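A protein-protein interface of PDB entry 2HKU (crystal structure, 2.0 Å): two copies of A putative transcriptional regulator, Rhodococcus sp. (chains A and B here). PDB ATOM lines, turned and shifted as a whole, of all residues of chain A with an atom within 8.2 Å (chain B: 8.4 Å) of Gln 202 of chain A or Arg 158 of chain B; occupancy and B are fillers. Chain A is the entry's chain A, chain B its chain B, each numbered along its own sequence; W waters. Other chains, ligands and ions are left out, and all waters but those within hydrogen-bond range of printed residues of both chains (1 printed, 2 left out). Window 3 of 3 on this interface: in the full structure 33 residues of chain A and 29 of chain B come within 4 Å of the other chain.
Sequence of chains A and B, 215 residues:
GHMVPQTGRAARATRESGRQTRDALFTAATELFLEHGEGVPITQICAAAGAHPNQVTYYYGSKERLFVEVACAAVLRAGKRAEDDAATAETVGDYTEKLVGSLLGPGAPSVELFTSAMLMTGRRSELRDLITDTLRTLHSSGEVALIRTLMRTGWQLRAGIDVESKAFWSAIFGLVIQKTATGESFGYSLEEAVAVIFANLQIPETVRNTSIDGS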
ATOM      1  N   LEU A 150     -21.204  -8.750 -10.888  1.00  0.00           N
ATOM      2  CA  LEU A 150     -20.825  -8.341  -9.553  1.00  0.00           C
ATOM      3  C   LEU A 150     -21.756  -8.783  -8.444  1.00  0.00           C
ATOM      4  O   LEU A 150     -21.301  -9.209  -7.383  1.00  0.00           O
ATOM      5  CB  LEU A 150     -20.676  -6.799  -9.463  1.00  0.00           C
ATOM      6  CG  LEU A 150     -19.627  -6.074 -10.310  1.00  0.00           C
ATOM      7  CD1 LEU A 150     -19.582  -4.537  -9.882  1.00  0.00           C
ATOM      8  CD2 LEU A 150     -18.259  -6.717 -10.213  1.00  0.00           C
ATOM      9  N   TRP A 155     -20.757  -8.795  -4.612  1.00  0.00           N
ATOM     10  CA  TRP A 155     -20.660  -7.318  -4.454  1.00  0.00           C
ATOM     11  C   TRP A 155     -21.981  -6.666  -3.972  1.00  0.00           C
ATOM     12  O   TRP A 155     -23.059  -7.044  -4.432  1.00  0.00           O
ATOM     13  CB  TRP A 155     -20.105  -6.765  -5.804  1.00  0.00           C
ATOM     14  CG  TRP A 155     -19.915  -5.288  -5.967  1.00  0.00           C
ATOM     15  CD1 TRP A 155     -18.773  -4.530  -5.686  1.00  0.00           C
ATOM     16  CD2 TRP A 155     -20.879  -4.367  -6.537  1.00  0.00           C
ATOM     17  NE1 TRP A 155     -19.005  -3.214  -6.033  1.00  0.00           N
ATOM     18  CE2 TRP A 155     -20.270  -3.087  -6.561  1.00  0.00           C
ATOM     19  CE3 TRP A 155     -22.201  -4.509  -7.009  1.00  0.00           C
ATOM     20  CZ2 TRP A 155     -20.949  -1.948  -7.022  1.00  0.00           C
ATOM     21  CZ3 TRP A 155     -22.867  -3.377  -7.493  1.00  0.00           C
ATOM     22  CH2 TRP A 155     -22.239  -2.111  -7.480  1.00  0.00           C
ATOM     23  N   GLN A 156     -21.910  -5.751  -3.008  1.00  0.00           N
ATOM     24  CA  GLN A 156     -23.066  -5.074  -2.522  1.00  0.00           C
ATOM     25  C   GLN A 156     -23.353  -3.770  -3.311  1.00  0.00           C
ATOM     26  O   GLN A 156     -22.500  -2.846  -3.345  1.00  0.00           O
ATOM     27  CB  GLN A 156     -22.907  -4.643  -1.059  1.00  0.00           C
ATOM     28  CG  GLN A 156     -22.719  -5.763  -0.003  1.00  0.00           C
ATOM     29  CD  GLN A 156     -23.842  -6.771  -0.025  1.00  0.00           C
ATOM     30  OE1 GLN A 156     -24.924  -6.546   0.578  1.00  0.00           O
ATOM     31  NE2 GLN A 156     -23.618  -7.889  -0.748  1.00  0.00           N
ATOM     32  N   ARG A 158     -24.637  -0.168  -3.792  1.00  0.00           N
ATOM     33  CA  ARG A 158     -24.587   0.999  -2.947  1.00  0.00           C
ATOM     34  C   ARG A 158     -25.865   1.798  -3.216  1.00  0.00           C
ATOM     35  O   ARG A 158     -26.303   2.588  -2.412  1.00  0.00           O
ATOM     36  CB  ARG A 158     -23.341   1.863  -3.303  1.00  0.00           C
ATOM     37  CG  ARG A 158     -21.991   1.321  -2.925  1.00  0.00           C
ATOM     38  CD  ARG A 158     -21.490   0.323  -3.944  1.00  0.00           C
ATOM     39  NE  ARG A 158     -21.459   0.940  -5.297  1.00  0.00           N
ATOM     40  CZ  ARG A 158     -20.349   1.376  -5.875  1.00  0.00           C
ATOM     41  NH1 ARG A 158     -20.451   1.920  -7.083  1.00  0.00           N
ATOM     42  NH2 ARG A 158     -19.128   1.269  -5.258  1.00  0.00           N
ATOM     43  N   ALA A 195      -8.255   2.706 -13.563  1.00  0.00           N
ATOM     44  CA  ALA A 195      -8.217   2.798 -12.098  1.00  0.00           C
ATOM     45  C   ALA A 195      -9.364   3.654 -11.501  1.00  0.00           C
ATOM     46  O   ALA A 195      -9.833   3.409 -10.400  1.00  0.00           O
ATOM     47  CB  ALA A 195      -6.849   3.328 -11.626  1.00  0.00           C
ATOM     48  N   VAL A 196      -9.825   4.673 -12.214  1.00  0.00           N
ATOM     49  CA  VAL A 196     -10.994   5.472 -11.673  1.00  0.00           C
ATOM     50  C   VAL A 196     -12.226   4.500 -11.616  1.00  0.00           C
ATOM     51  O   VAL A 196     -12.939   4.478 -10.633  1.00  0.00           O
ATOM     52  CB  VAL A 196     -11.307   6.752 -12.577  1.00  0.00           C
ATOM     53  CG1 VAL A 196     -12.697   7.254 -12.362  1.00  0.00           C
ATOM     54  CG2 VAL A 196     -10.211   7.928 -12.388  1.00  0.00           C
ATOM     55  N   ILE A 197     -12.450   3.694 -12.658  1.00  0.00           N
ATOM     56  CA  ILE A 197     -13.647   2.782 -12.647  1.00  0.00           C
ATOM     57  C   ILE A 197     -13.498   1.787 -11.498  1.00  0.00           C
ATOM     58  O   ILE A 197     -14.428   1.635 -10.709  1.00  0.00           O
ATOM     59  CB  ILE A 197     -13.884   2.034 -13.963  1.00  0.00           C
ATOM     60  CG1 ILE A 197     -14.195   2.962 -15.169  1.00  0.00           C
ATOM     61  CG2 ILE A 197     -15.021   0.950 -13.811  1.00  0.00           C
ATOM     62  CD1 ILE A 197     -15.536   3.732 -15.071  1.00  0.00           C
ATOM     63  N   PHE A 198     -12.297   1.177 -11.353  1.00  0.00           N
ATOM     64  CA  PHE A 198     -12.045   0.383 -10.111  1.00  0.00           C
ATOM     65  C   PHE A 198     -12.296   1.057  -8.757  1.00  0.00           C
ATOM     66  O   PHE A 198     -12.859   0.434  -7.836  1.00  0.00           O
ATOM     67  CB  PHE A 198     -10.701  -0.346 -10.209  1.00  0.00           C
ATOM     68  CG  PHE A 198     -10.755  -1.510 -11.155  1.00  0.00           C
ATOM     69  CD1 PHE A 198     -11.323  -2.726 -10.734  1.00  0.00           C
ATOM     70  CD2 PHE A 198     -10.304  -1.402 -12.445  1.00  0.00           C
ATOM     71  CE1 PHE A 198     -11.424  -3.833 -11.588  1.00  0.00           C
ATOM     72  CE2 PHE A 198     -10.393  -2.498 -13.347  1.00  0.00           C
ATOM     73  CZ  PHE A 198     -10.957  -3.718 -12.897  1.00  0.00           C
ATOM     74  N   ALA A 199     -11.877   2.321  -8.600  1.00  0.00           N
ATOM     75  CA  ALA A 199     -12.211   3.080  -7.415  1.00  0.00           C
ATOM     76  C   ALA A 199     -13.673   3.382  -7.291  1.00  0.00           C
ATOM     77  O   ALA A 199     -14.192   3.445  -6.153  1.00  0.00           O
ATOM     78  CB  ALA A 199     -11.391   4.395  -7.352  1.00  0.00           C
ATOM     79  N   ASN A 200     -14.379   3.575  -8.422  1.00  0.00           N
ATOM     80  CA  ASN A 200     -15.838   3.802  -8.357  1.00  0.00           C
ATOM     81  C   ASN A 200     -16.590   2.544  -7.870  1.00  0.00           C
ATOM     82  O   ASN A 200     -17.569   2.655  -7.194  1.00  0.00           O
ATOM     83  CB  ASN A 200     -16.412   4.169  -9.754  1.00  0.00           C
ATOM     84  CG  ASN A 200     -16.018   5.576 -10.229  1.00  0.00           C
ATOM     85  OD1 ASN A 200     -16.214   5.921 -11.407  1.00  0.00           O
ATOM     86  ND2 ASN A 200     -15.484   6.360  -9.364  1.00  0.00           N
ATOM     87  N   LEU A 201     -16.137   1.364  -8.303  1.00  0.00           N
ATOM     88  CA  LEU A 201     -16.834   0.086  -8.022  1.00  0.00           C
ATOM     89  C   LEU A 201     -16.424  -0.480  -6.652  1.00  0.00           C
ATOM     90  O   LEU A 201     -17.239  -1.133  -6.006  1.00  0.00           O
ATOM     91  CB  LEU A 201     -16.518  -0.913  -9.116  1.00  0.00           C
ATOM     92  CG  LEU A 201     -17.086  -0.518 -10.495  1.00  0.00           C
ATOM     93  CD1 LEU A 201     -16.578  -1.416 -11.585  1.00  0.00           C
ATOM     94  CD2 LEU A 201     -18.618  -0.571 -10.381  1.00  0.00           C
ATOM     95  N   GLN A 202     -15.171  -0.201  -6.244  1.00  0.00           N
ATOM     96  CA  GLN A 202     -14.544  -0.671  -4.979  1.00  0.00           C
ATOM     97  C   GLN A 202     -14.951  -2.158  -4.713  1.00  0.00           C
ATOM     98  O   GLN A 202     -15.774  -2.430  -3.867  1.00  0.00           O
ATOM     99  CB  GLN A 202     -14.960   0.270  -3.851  1.00  0.00           C
ATOM    100  CG  GLN A 202     -13.908   0.473  -2.772  1.00  0.00           C
ATOM    101  CD  GLN A 202     -12.557   0.983  -3.344  1.00  0.00           C
ATOM    102  OE1 GLN A 202     -11.607   0.194  -3.484  1.00  0.00           O
ATOM    103  NE2 GLN A 202     -12.483   2.291  -3.698  1.00  0.00           N
ATOM    104  N   ILE A 203     -14.444  -3.061  -5.532  1.00  0.00           N
ATOM    105  CA  ILE A 203     -14.859  -4.452  -5.580  1.00  0.00           C
ATOM    106  C   ILE A 203     -13.903  -5.159  -4.611  1.00  0.00           C
ATOM    107  O   ILE A 203     -12.686  -5.147  -4.875  1.00  0.00           O
ATOM    108  CB  ILE A 203     -14.578  -5.083  -6.969  1.00  0.00           C
ATOM    109  CG1 ILE A 203     -15.304  -4.358  -8.096  1.00  0.00           C
ATOM    110  CG2 ILE A 203     -14.964  -6.610  -6.973  1.00  0.00           C
ATOM    111  CD1 ILE A 203     -14.996  -4.930  -9.460  1.00  0.00           C
ATOM    112  N   PRO A 204     -14.448  -5.759  -3.515  1.00  0.00           N
ATOM    113  CA  PRO A 204     -13.637  -6.570  -2.576  1.00  0.00           C
ATOM    114  C   PRO A 204     -12.738  -7.580  -3.240  1.00  0.00           C
ATOM    115  O   PRO A 204     -13.106  -8.222  -4.255  1.00  0.00           O
ATOM    116  CB  PRO A 204     -14.681  -7.228  -1.683  1.00  0.00           C
ATOM    117  CG  PRO A 204     -15.849  -6.216  -1.617  1.00  0.00           C
ATOM    118  CD  PRO A 204     -15.867  -5.654  -3.072  1.00  0.00           C
ATOM    119  N   GLU A 205     -11.534  -7.735  -2.669  1.00  0.00           N
ATOM    120  CA  GLU A 205     -10.541  -8.619  -3.268  1.00  0.00           C
ATOM    121  C   GLU A 205     -11.085 -10.053  -3.487  1.00  0.00           C
ATOM    122  O   GLU A 205     -10.755 -10.689  -4.478  1.00  0.00           O
ATOM    123  CB  GLU A 205      -9.230  -8.632  -2.463  1.00  0.00           C
ATOM    124  CG  GLU A 205      -8.034  -8.942  -3.322  1.00  0.00           C
ATOM    125  CD  GLU A 205      -6.755  -9.221  -2.523  1.00  0.00           C
ATOM    126  OE1 GLU A 205      -6.611  -8.649  -1.403  1.00  0.00           O
ATOM    127  OE2 GLU A 205      -5.900 -10.029  -3.018  1.00  0.00           O
ATOM    128  N   VAL A 207     -14.363 -11.168  -3.910  1.00  0.00           N
ATOM    129  CA  VAL A 207     -15.157 -10.996  -5.151  1.00  0.00           C
ATOM    130  C   VAL A 207     -14.304 -10.944  -6.415  1.00  0.00           C
ATOM    131  O   VAL A 207     -14.600 -11.647  -7.352  1.00  0.00           O
ATOM    132  CB  VAL A 207     -16.050  -9.765  -5.061  1.00  0.00           C
ATOM    133  CG1 VAL A 207     -16.978  -9.671  -6.312  1.00  0.00           C
ATOM    134  CG2 VAL A 207     -16.836  -9.770  -3.744  1.00  0.00           C
ATOM    135  N   ARG A 208     -13.211 -10.163  -6.435  1.00  0.00           N
ATOM    136  CA  ARG A 208     -12.372 -10.050  -7.638  1.00  0.00           C
ATOM    137  C   ARG A 208     -11.727 -11.349  -8.021  1.00  0.00           C
ATOM    138  O   ARG A 208     -11.406 -11.588  -9.188  1.00  0.00           O
ATOM    139  CB  ARG A 208     -11.282  -8.968  -7.509  1.00  0.00           C
ATOM    140  CG  ARG A 208     -11.781  -7.544  -7.250  1.00  0.00           C
ATOM    141  CD  ARG A 208     -10.736  -6.444  -7.650  1.00  0.00           C
ATOM    142  NE  ARG A 208      -9.475  -6.495  -6.886  1.00  0.00           N
ATOM    143  CZ  ARG A 208      -9.265  -5.966  -5.674  1.00  0.00           C
ATOM    144  NH1 ARG A 208     -10.210  -5.298  -5.013  1.00  0.00           N
ATOM    145  NH2 ARG A 208      -8.071  -6.102  -5.114  1.00  0.00           N
ATOM    146  N   LEU B 150     -15.152  17.309   4.059  1.00  0.00           N
ATOM    147  CA  LEU B 150     -15.113  16.117   4.887  1.00  0.00           C
ATOM    148  C   LEU B 150     -14.323  16.287   6.207  1.00  0.00           C
ATOM    149  O   LEU B 150     -14.327  15.387   7.073  1.00  0.00           O
ATOM    150  CB  LEU B 150     -14.509  14.997   4.044  1.00  0.00           C
ATOM    151  CG  LEU B 150     -15.353  14.490   2.893  1.00  0.00           C
ATOM    152  CD1 LEU B 150     -14.643  13.420   2.042  1.00  0.00           C
ATOM    153  CD2 LEU B 150     -16.708  13.958   3.443  1.00  0.00           C
ATOM    154  N   GLY B 154     -14.277  13.169  10.083  1.00  0.00           N
ATOM    155  CA  GLY B 154     -13.420  12.041  10.484  1.00  0.00           C
ATOM    156  C   GLY B 154     -13.568  10.789   9.635  1.00  0.00           C
ATOM    157  O   GLY B 154     -13.023   9.702   9.965  1.00  0.00           O
ATOM    158  N   TRP B 155     -14.321  10.953   8.536  1.00  0.00           N
ATOM    159  CA  TRP B 155     -14.440   9.979   7.445  1.00  0.00           C
ATOM    160  C   TRP B 155     -13.432  10.219   6.327  1.00  0.00           C
ATOM    161  O   TRP B 155     -13.280  11.345   5.830  1.00  0.00           O
ATOM    162  CB  TRP B 155     -15.862   9.998   6.839  1.00  0.00           C
ATOM    163  CG  TRP B 155     -16.058   8.837   5.882  1.00  0.00           C
ATOM    164  CD1 TRP B 155     -16.251   7.519   6.215  1.00  0.00           C
ATOM    165  CD2 TRP B 155     -16.056   8.897   4.453  1.00  0.00           C
ATOM    166  NE1 TRP B 155     -16.372   6.757   5.082  1.00  0.00           N
ATOM    167  CE2 TRP B 155     -16.253   7.567   3.982  1.00  0.00           C
ATOM    168  CE3 TRP B 155     -15.893   9.942   3.517  1.00  0.00           C
ATOM    169  CZ2 TRP B 155     -16.301   7.246   2.604  1.00  0.00           C
ATOM    170  CZ3 TRP B 155     -15.946   9.633   2.144  1.00  0.00           C
ATOM    171  CH2 TRP B 155     -16.155   8.296   1.700  1.00  0.00           C
ATOM    172  N   GLN B 156     -12.802   9.136   5.896  1.00  0.00           N
ATOM    173  CA  GLN B 156     -11.767   9.181   4.924  1.00  0.00           C
ATOM    174  C   GLN B 156     -12.231   8.508   3.604  1.00  0.00           C
ATOM    175  O   GLN B 156     -12.776   7.388   3.567  1.00  0.00           O
ATOM    176  CB  GLN B 156     -10.550   8.477   5.494  1.00  0.00           C
ATOM    177  CG  GLN B 156      -9.224   9.108   5.185  1.00  0.00           C
ATOM    178  CD  GLN B 156      -8.087   8.080   5.152  1.00  0.00           C
ATOM    179  OE1 GLN B 156      -7.870   7.347   6.141  1.00  0.00           O
ATOM    180  NE2 GLN B 156      -7.348   8.029   4.006  1.00  0.00           N
ATOM    181  N   LEU B 157     -11.987   9.211   2.516  1.00  0.00           N
ATOM    182  CA  LEU B 157     -12.354   8.756   1.227  1.00  0.00           C
ATOM    183  C   LEU B 157     -11.658   7.464   0.994  1.00  0.00           C
ATOM    184  O   LEU B 157     -10.592   7.258   1.552  1.00  0.00           O
ATOM    185  CB  LEU B 157     -11.823   9.754   0.188  1.00  0.00           C
ATOM    186  CG  LEU B 157     -12.542  11.073   0.028  1.00  0.00           C
ATOM    187  CD1 LEU B 157     -11.532  11.970  -0.705  1.00  0.00           C
ATOM    188  CD2 LEU B 157     -13.842  10.938  -0.757  1.00  0.00           C
ATOM    189  N   ARG B 158     -12.237   6.625   0.133  1.00  0.00           N
ATOM    190  CA  ARG B 158     -11.751   5.264  -0.125  1.00  0.00           C
ATOM    191  C   ARG B 158     -10.577   5.168  -1.046  1.00  0.00           C
ATOM    192  O   ARG B 158      -9.706   4.327  -0.821  1.00  0.00           O
ATOM    193  CB  ARG B 158     -12.887   4.326  -0.633  1.00  0.00           C
ATOM    194  CG  ARG B 158     -14.170   4.300   0.305  1.00  0.00           C
ATOM    195  CD  ARG B 158     -13.789   3.757   1.686  1.00  0.00           C
ATOM    196  NE  ARG B 158     -14.210   4.601   2.848  1.00  0.00           N
ATOM    197  CZ  ARG B 158     -13.491   4.736   3.980  1.00  0.00           C
ATOM    198  NH1 ARG B 158     -12.311   4.155   4.113  1.00  0.00           N
ATOM    199  NH2 ARG B 158     -13.921   5.478   4.988  1.00  0.00           N
ATOM    200  N   ALA B 159     -10.491   6.009  -2.087  1.00  0.00           N
ATOM    201  CA  ALA B 159      -9.303   5.992  -2.835  1.00  0.00           C
ATOM    202  C   ALA B 159      -8.568   7.335  -2.594  1.00  0.00           C
ATOM    203  O   ALA B 159      -9.086   8.252  -1.906  1.00  0.00           O
ATOM    204  CB  ALA B 159      -9.636   5.779  -4.328  1.00  0.00           C
ATOM    205  N   GLY B 160      -7.404   7.464  -3.217  1.00  0.00           N
ATOM    206  CA  GLY B 160      -6.633   8.716  -3.242  1.00  0.00           C
ATOM    207  C   GLY B 160      -7.480   9.942  -3.596  1.00  0.00           C
ATOM    208  O   GLY B 160      -8.330   9.906  -4.532  1.00  0.00           O
ATOM    209  N   ILE B 161      -7.221  11.053  -2.915  1.00  0.00           N
ATOM    210  CA  ILE B 161      -7.946  12.316  -3.219  1.00  0.00           C
ATOM    211  C   ILE B 161      -7.888  12.707  -4.712  1.00  0.00           C
ATOM    212  O   ILE B 161      -8.858  13.223  -5.213  1.00  0.00           O
ATOM    213  CB  ILE B 161      -7.584  13.444  -2.276  1.00  0.00           C
ATOM    214  CG1 ILE B 161      -8.553  14.611  -2.365  1.00  0.00           C
ATOM    215  CG2 ILE B 161      -6.133  13.993  -2.471  1.00  0.00           C
ATOM    216  CD1 ILE B 161      -9.964  14.296  -2.226  1.00  0.00           C
ATOM    217  N   VAL B 163      -7.773  10.604  -7.260  1.00  0.00           N
ATOM    218  CA  VAL B 163      -8.575   9.612  -7.988  1.00  0.00           C
ATOM    219  C   VAL B 163     -10.016  10.017  -7.732  1.00  0.00           C
ATOM    220  O   VAL B 163     -10.799   9.993  -8.665  1.00  0.00           O
ATOM    221  CB  VAL B 163      -8.278   8.118  -7.573  1.00  0.00           C
ATOM    222  CG1 VAL B 163      -9.296   7.179  -8.270  1.00  0.00           C
ATOM    223  CG2 VAL B 163      -6.849   7.715  -7.961  1.00  0.00           C
ATOM    224  N   GLU B 164     -10.328  10.457  -6.524  1.00  0.00           N
ATOM    225  CA  GLU B 164     -11.692  10.881  -6.217  1.00  0.00           C
ATOM    226  C   GLU B 164     -12.158  12.126  -6.999  1.00  0.00           C
ATOM    227  O   GLU B 164     -13.331  12.256  -7.326  1.00  0.00           O
ATOM    228  CB  GLU B 164     -11.860  11.106  -4.727  1.00  0.00           C
ATOM    229  CG  GLU B 164     -11.718   9.825  -3.820  1.00  0.00           C
ATOM    230  CD  GLU B 164     -12.887   8.764  -3.941  1.00  0.00           C
ATOM    231  OE1 GLU B 164     -13.650   8.729  -4.916  1.00  0.00           O
ATOM    232  OE2 GLU B 164     -13.010   7.922  -3.048  1.00  0.00           O
ATOM    233  N   ALA B 199     -22.588   7.033  -4.771  1.00  0.00           N
ATOM    234  CA  ALA B 199     -22.101   5.632  -5.028  1.00  0.00           C
ATOM    235  C   ALA B 199     -20.603   5.508  -5.409  1.00  0.00           C
ATOM    236  O   ALA B 199     -19.840   4.648  -4.894  1.00  0.00           O
ATOM    237  CB  ALA B 199     -22.953   4.968  -6.103  1.00  0.00           C
ATOM    238  N   ASN B 200     -20.200   6.318  -6.374  1.00  0.00           N
ATOM    239  CA  ASN B 200     -18.824   6.349  -6.847  1.00  0.00           C
ATOM    240  C   ASN B 200     -17.838   6.665  -5.768  1.00  0.00           C
ATOM    241  O   ASN B 200     -16.738   6.166  -5.806  1.00  0.00           O
ATOM    242  CB  ASN B 200     -18.677   7.256  -8.083  1.00  0.00           C
ATOM    243  CG  ASN B 200     -19.305   6.629  -9.310  1.00  0.00           C
ATOM    244  OD1 ASN B 200     -19.654   5.447  -9.305  1.00  0.00           O
ATOM    245  ND2 ASN B 200     -19.495   7.422 -10.348  1.00  0.00           N
ATOM    246  N   LEU B 201     -18.283   7.411  -4.769  1.00  0.00           N
ATOM    247  CA  LEU B 201     -17.455   7.793  -3.655  1.00  0.00           C
ATOM    248  C   LEU B 201     -17.697   6.912  -2.407  1.00  0.00           C
ATOM    249  O   LEU B 201     -16.996   7.048  -1.397  1.00  0.00           O
ATOM    250  CB  LEU B 201     -17.687   9.292  -3.340  1.00  0.00           C
ATOM    251  CG  LEU B 201     -16.964  10.201  -4.362  1.00  0.00           C
ATOM    252  CD1 LEU B 201     -17.568  10.238  -5.891  1.00  0.00           C
ATOM    253  CD2 LEU B 201     -16.684  11.602  -3.788  1.00  0.00           C
ATOM    254  N   GLN B 202     -18.680   6.012  -2.482  1.00  0.00           N
ATOM    255  CA  GLN B 202     -19.148   5.246  -1.294  1.00  0.00           C
ATOM    256  C   GLN B 202     -19.270   6.094  -0.028  1.00  0.00           C
ATOM    257  O   GLN B 202     -18.746   5.715   1.023  1.00  0.00           O
ATOM    258  CB  GLN B 202     -18.214   4.051  -1.007  1.00  0.00           C
ATOM    259  CG  GLN B 202     -18.033   3.152  -2.171  1.00  0.00           C
ATOM    260  CD  GLN B 202     -16.892   3.563  -3.013  1.00  0.00           C
ATOM    261  OE1 GLN B 202     -15.809   3.927  -2.512  1.00  0.00           O
ATOM    262  NE2 GLN B 202     -17.095   3.517  -4.326  1.00  0.00           N
ATOM    263  N   ILE B 203     -19.927   7.249  -0.095  1.00  0.00           N
ATOM    264  CA  ILE B 203     -20.033   8.075   1.125  1.00  0.00           C
ATOM    265  C   ILE B 203     -21.189   7.487   1.938  1.00  0.00           C
ATOM    266  O   ILE B 203     -22.330   7.484   1.469  1.00  0.00           O
ATOM    267  CB  ILE B 203     -20.258   9.569   0.822  1.00  0.00           C
ATOM    268  CG1 ILE B 203     -19.108  10.135  -0.032  1.00  0.00           C
ATOM    269  CG2 ILE B 203     -20.257  10.398   2.092  1.00  0.00           C
ATOM    270  CD1 ILE B 203     -19.491  11.348  -0.995  1.00  0.00           C
ATOM    271  N   PRO B 204     -20.901   6.954   3.141  1.00  0.00           N
ATOM    272  CA  PRO B 204     -21.981   6.365   3.945  1.00  0.00           C
ATOM    273  C   PRO B 204     -23.091   7.392   4.254  1.00  0.00           C
ATOM    274  O   PRO B 204     -22.801   8.575   4.390  1.00  0.00           O
ATOM    275  CB  PRO B 204     -21.260   5.950   5.250  1.00  0.00           C
ATOM    276  CG  PRO B 204     -19.752   5.747   4.813  1.00  0.00           C
ATOM    277  CD  PRO B 204     -19.586   6.872   3.819  1.00  0.00           C
ATOM    278  N   VAL B 207     -22.323   9.885   7.200  1.00  0.00           N
ATOM    279  CA  VAL B 207     -21.382  10.908   6.696  1.00  0.00           C
ATOM    280  C   VAL B 207     -22.142  12.021   5.958  1.00  0.00           C
ATOM    281  O   VAL B 207     -21.957  13.186   6.255  1.00  0.00           O
ATOM    282  CB  VAL B 207     -20.222  10.263   5.866  1.00  0.00           C
ATOM    283  CG1 VAL B 207     -19.179  11.361   5.428  1.00  0.00           C
ATOM    284  CG2 VAL B 207     -19.535   9.181   6.730  1.00  0.00           C
HETATM  285  O   HOH W   1     -16.824   8.589 -12.233  1.00  0.00           O
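Ala 199 of chain A touches Asn 200 of chain B, and with the chains exchanged Asn 200 of chain A touches Ala 199 of chain B.
Ala 199 of chain A touches Gln 202 of chain B, but with the chains exchanged Gln 202 of chain A does not touch Ala 199 of chain B (6.6 Å).
Asn 200 of chain B touches its own counterpart, Asn 200 of chain A.
Asn 200 of chain A touches Gln 202 of chain B, but with the chains exchanged Gln 202 of chain A does not touch Asn 200 of chain B (6.1 Å).
Positions printed for both chains: 150, 155, 156, 158, 199, 200, 201, 202, 203, 204 and 207.
Of the 18 printed residues of chain B, 6 touch a printed residue of chain A.
Among the printed residues, 11 pairs touch across the chains.
Among the printed residues, no Asp or Glu carboxylate lies within 4 Å of a Lys or Arg side-chain nitrogen of the other chain.
O of Asn 200 of chain A is in hydrogen-bond range of NH2 of Arg 158 of chain A, 2.8 Å away.
NH2 of Arg 158 of chain A sits at hydrogen-bond distance from O of Leu 201 of chain A, at 3.1 Å.
The backbone carbonyl oxygen (O) of Val 196 of chain A lies close to the side-chain amide nitrogen (ND2) of Asn 200 of chain A, 3.4 Å away.
The backbone NH of Ala 159 of chain B lies within hydrogen-bond range of the side-chain carboxylate of Glu 164 of chain B (3.3 Å).
NE2 of Gln 202 of chain B sits at hydrogen-bond distance from O of Ala 199 of chain B, 3.0 Å away.
The side-chain amide nitrogen (NE2) of Gln 202 of chain B lies within hydrogen-bond range of the backbone carbonyl oxygen (O) of Asn 200 of chain B.
NH2 of Arg 158 of chain A sits close to O of Ala 199 of chain B (3.5 Å).
NH2 of Arg 158 of chain A lies close to NE2 of Gln 202 of chain B (3.2 Å).
O of Ala 199 of chain A is in hydrogen-bond range of NE2 of Gln 202 of chain B (3.4 Å).
O of Asn 200 of chain A sits at hydrogen-bond distance from NE2 of Gln 202 of chain B (3.0 Å).
Printed residues of chain B within 4 Å of Arg 158 of chain A: Ala 199 (3.5 Å) and Gln 202 (3.2 Å).
Gln 202 of chain A touches just these residues of chain B: Arg 158 and Gln 202.
Of chain A, only Gln 202 comes within 4 Å of Arg 158 of chain B.
Of chain A, only Ala 199 comes within 4 Å of Ala 159 of chain B.
Of the printed residues of chain A, Gln 202 of chain B touches Arg 158 (3.2 Å), Ala 199 (3.4 Å), Asn 200 (3.0 Å) and Gln 202 (3.9 Å).
Among the printed residues, merely in contact across the chains: Asn 200 of chain A with Asn 200 of chain B (3.5 Å), Ala 199 of chain A with Val 163 of chain B (3.6 Å), Gln 202 of chain A with Arg 158 of chain B (3.7 Å), Ala 199 of chain A with Asn 200 of chain B (3.7 Å), Ala 199 of chain A with Ala 159 of chain B (3.8 Å), Asn 200 of chain A with Ala 199 of chain B (3.8 Å) and Gln 202 of chain A with Gln 202 of chain B (3.9 Å).
Water W1 bridges OD1 of Asn 200 of chain A (2.9 Å) and ND2 of Asn 200 of chain B (3.5 Å).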
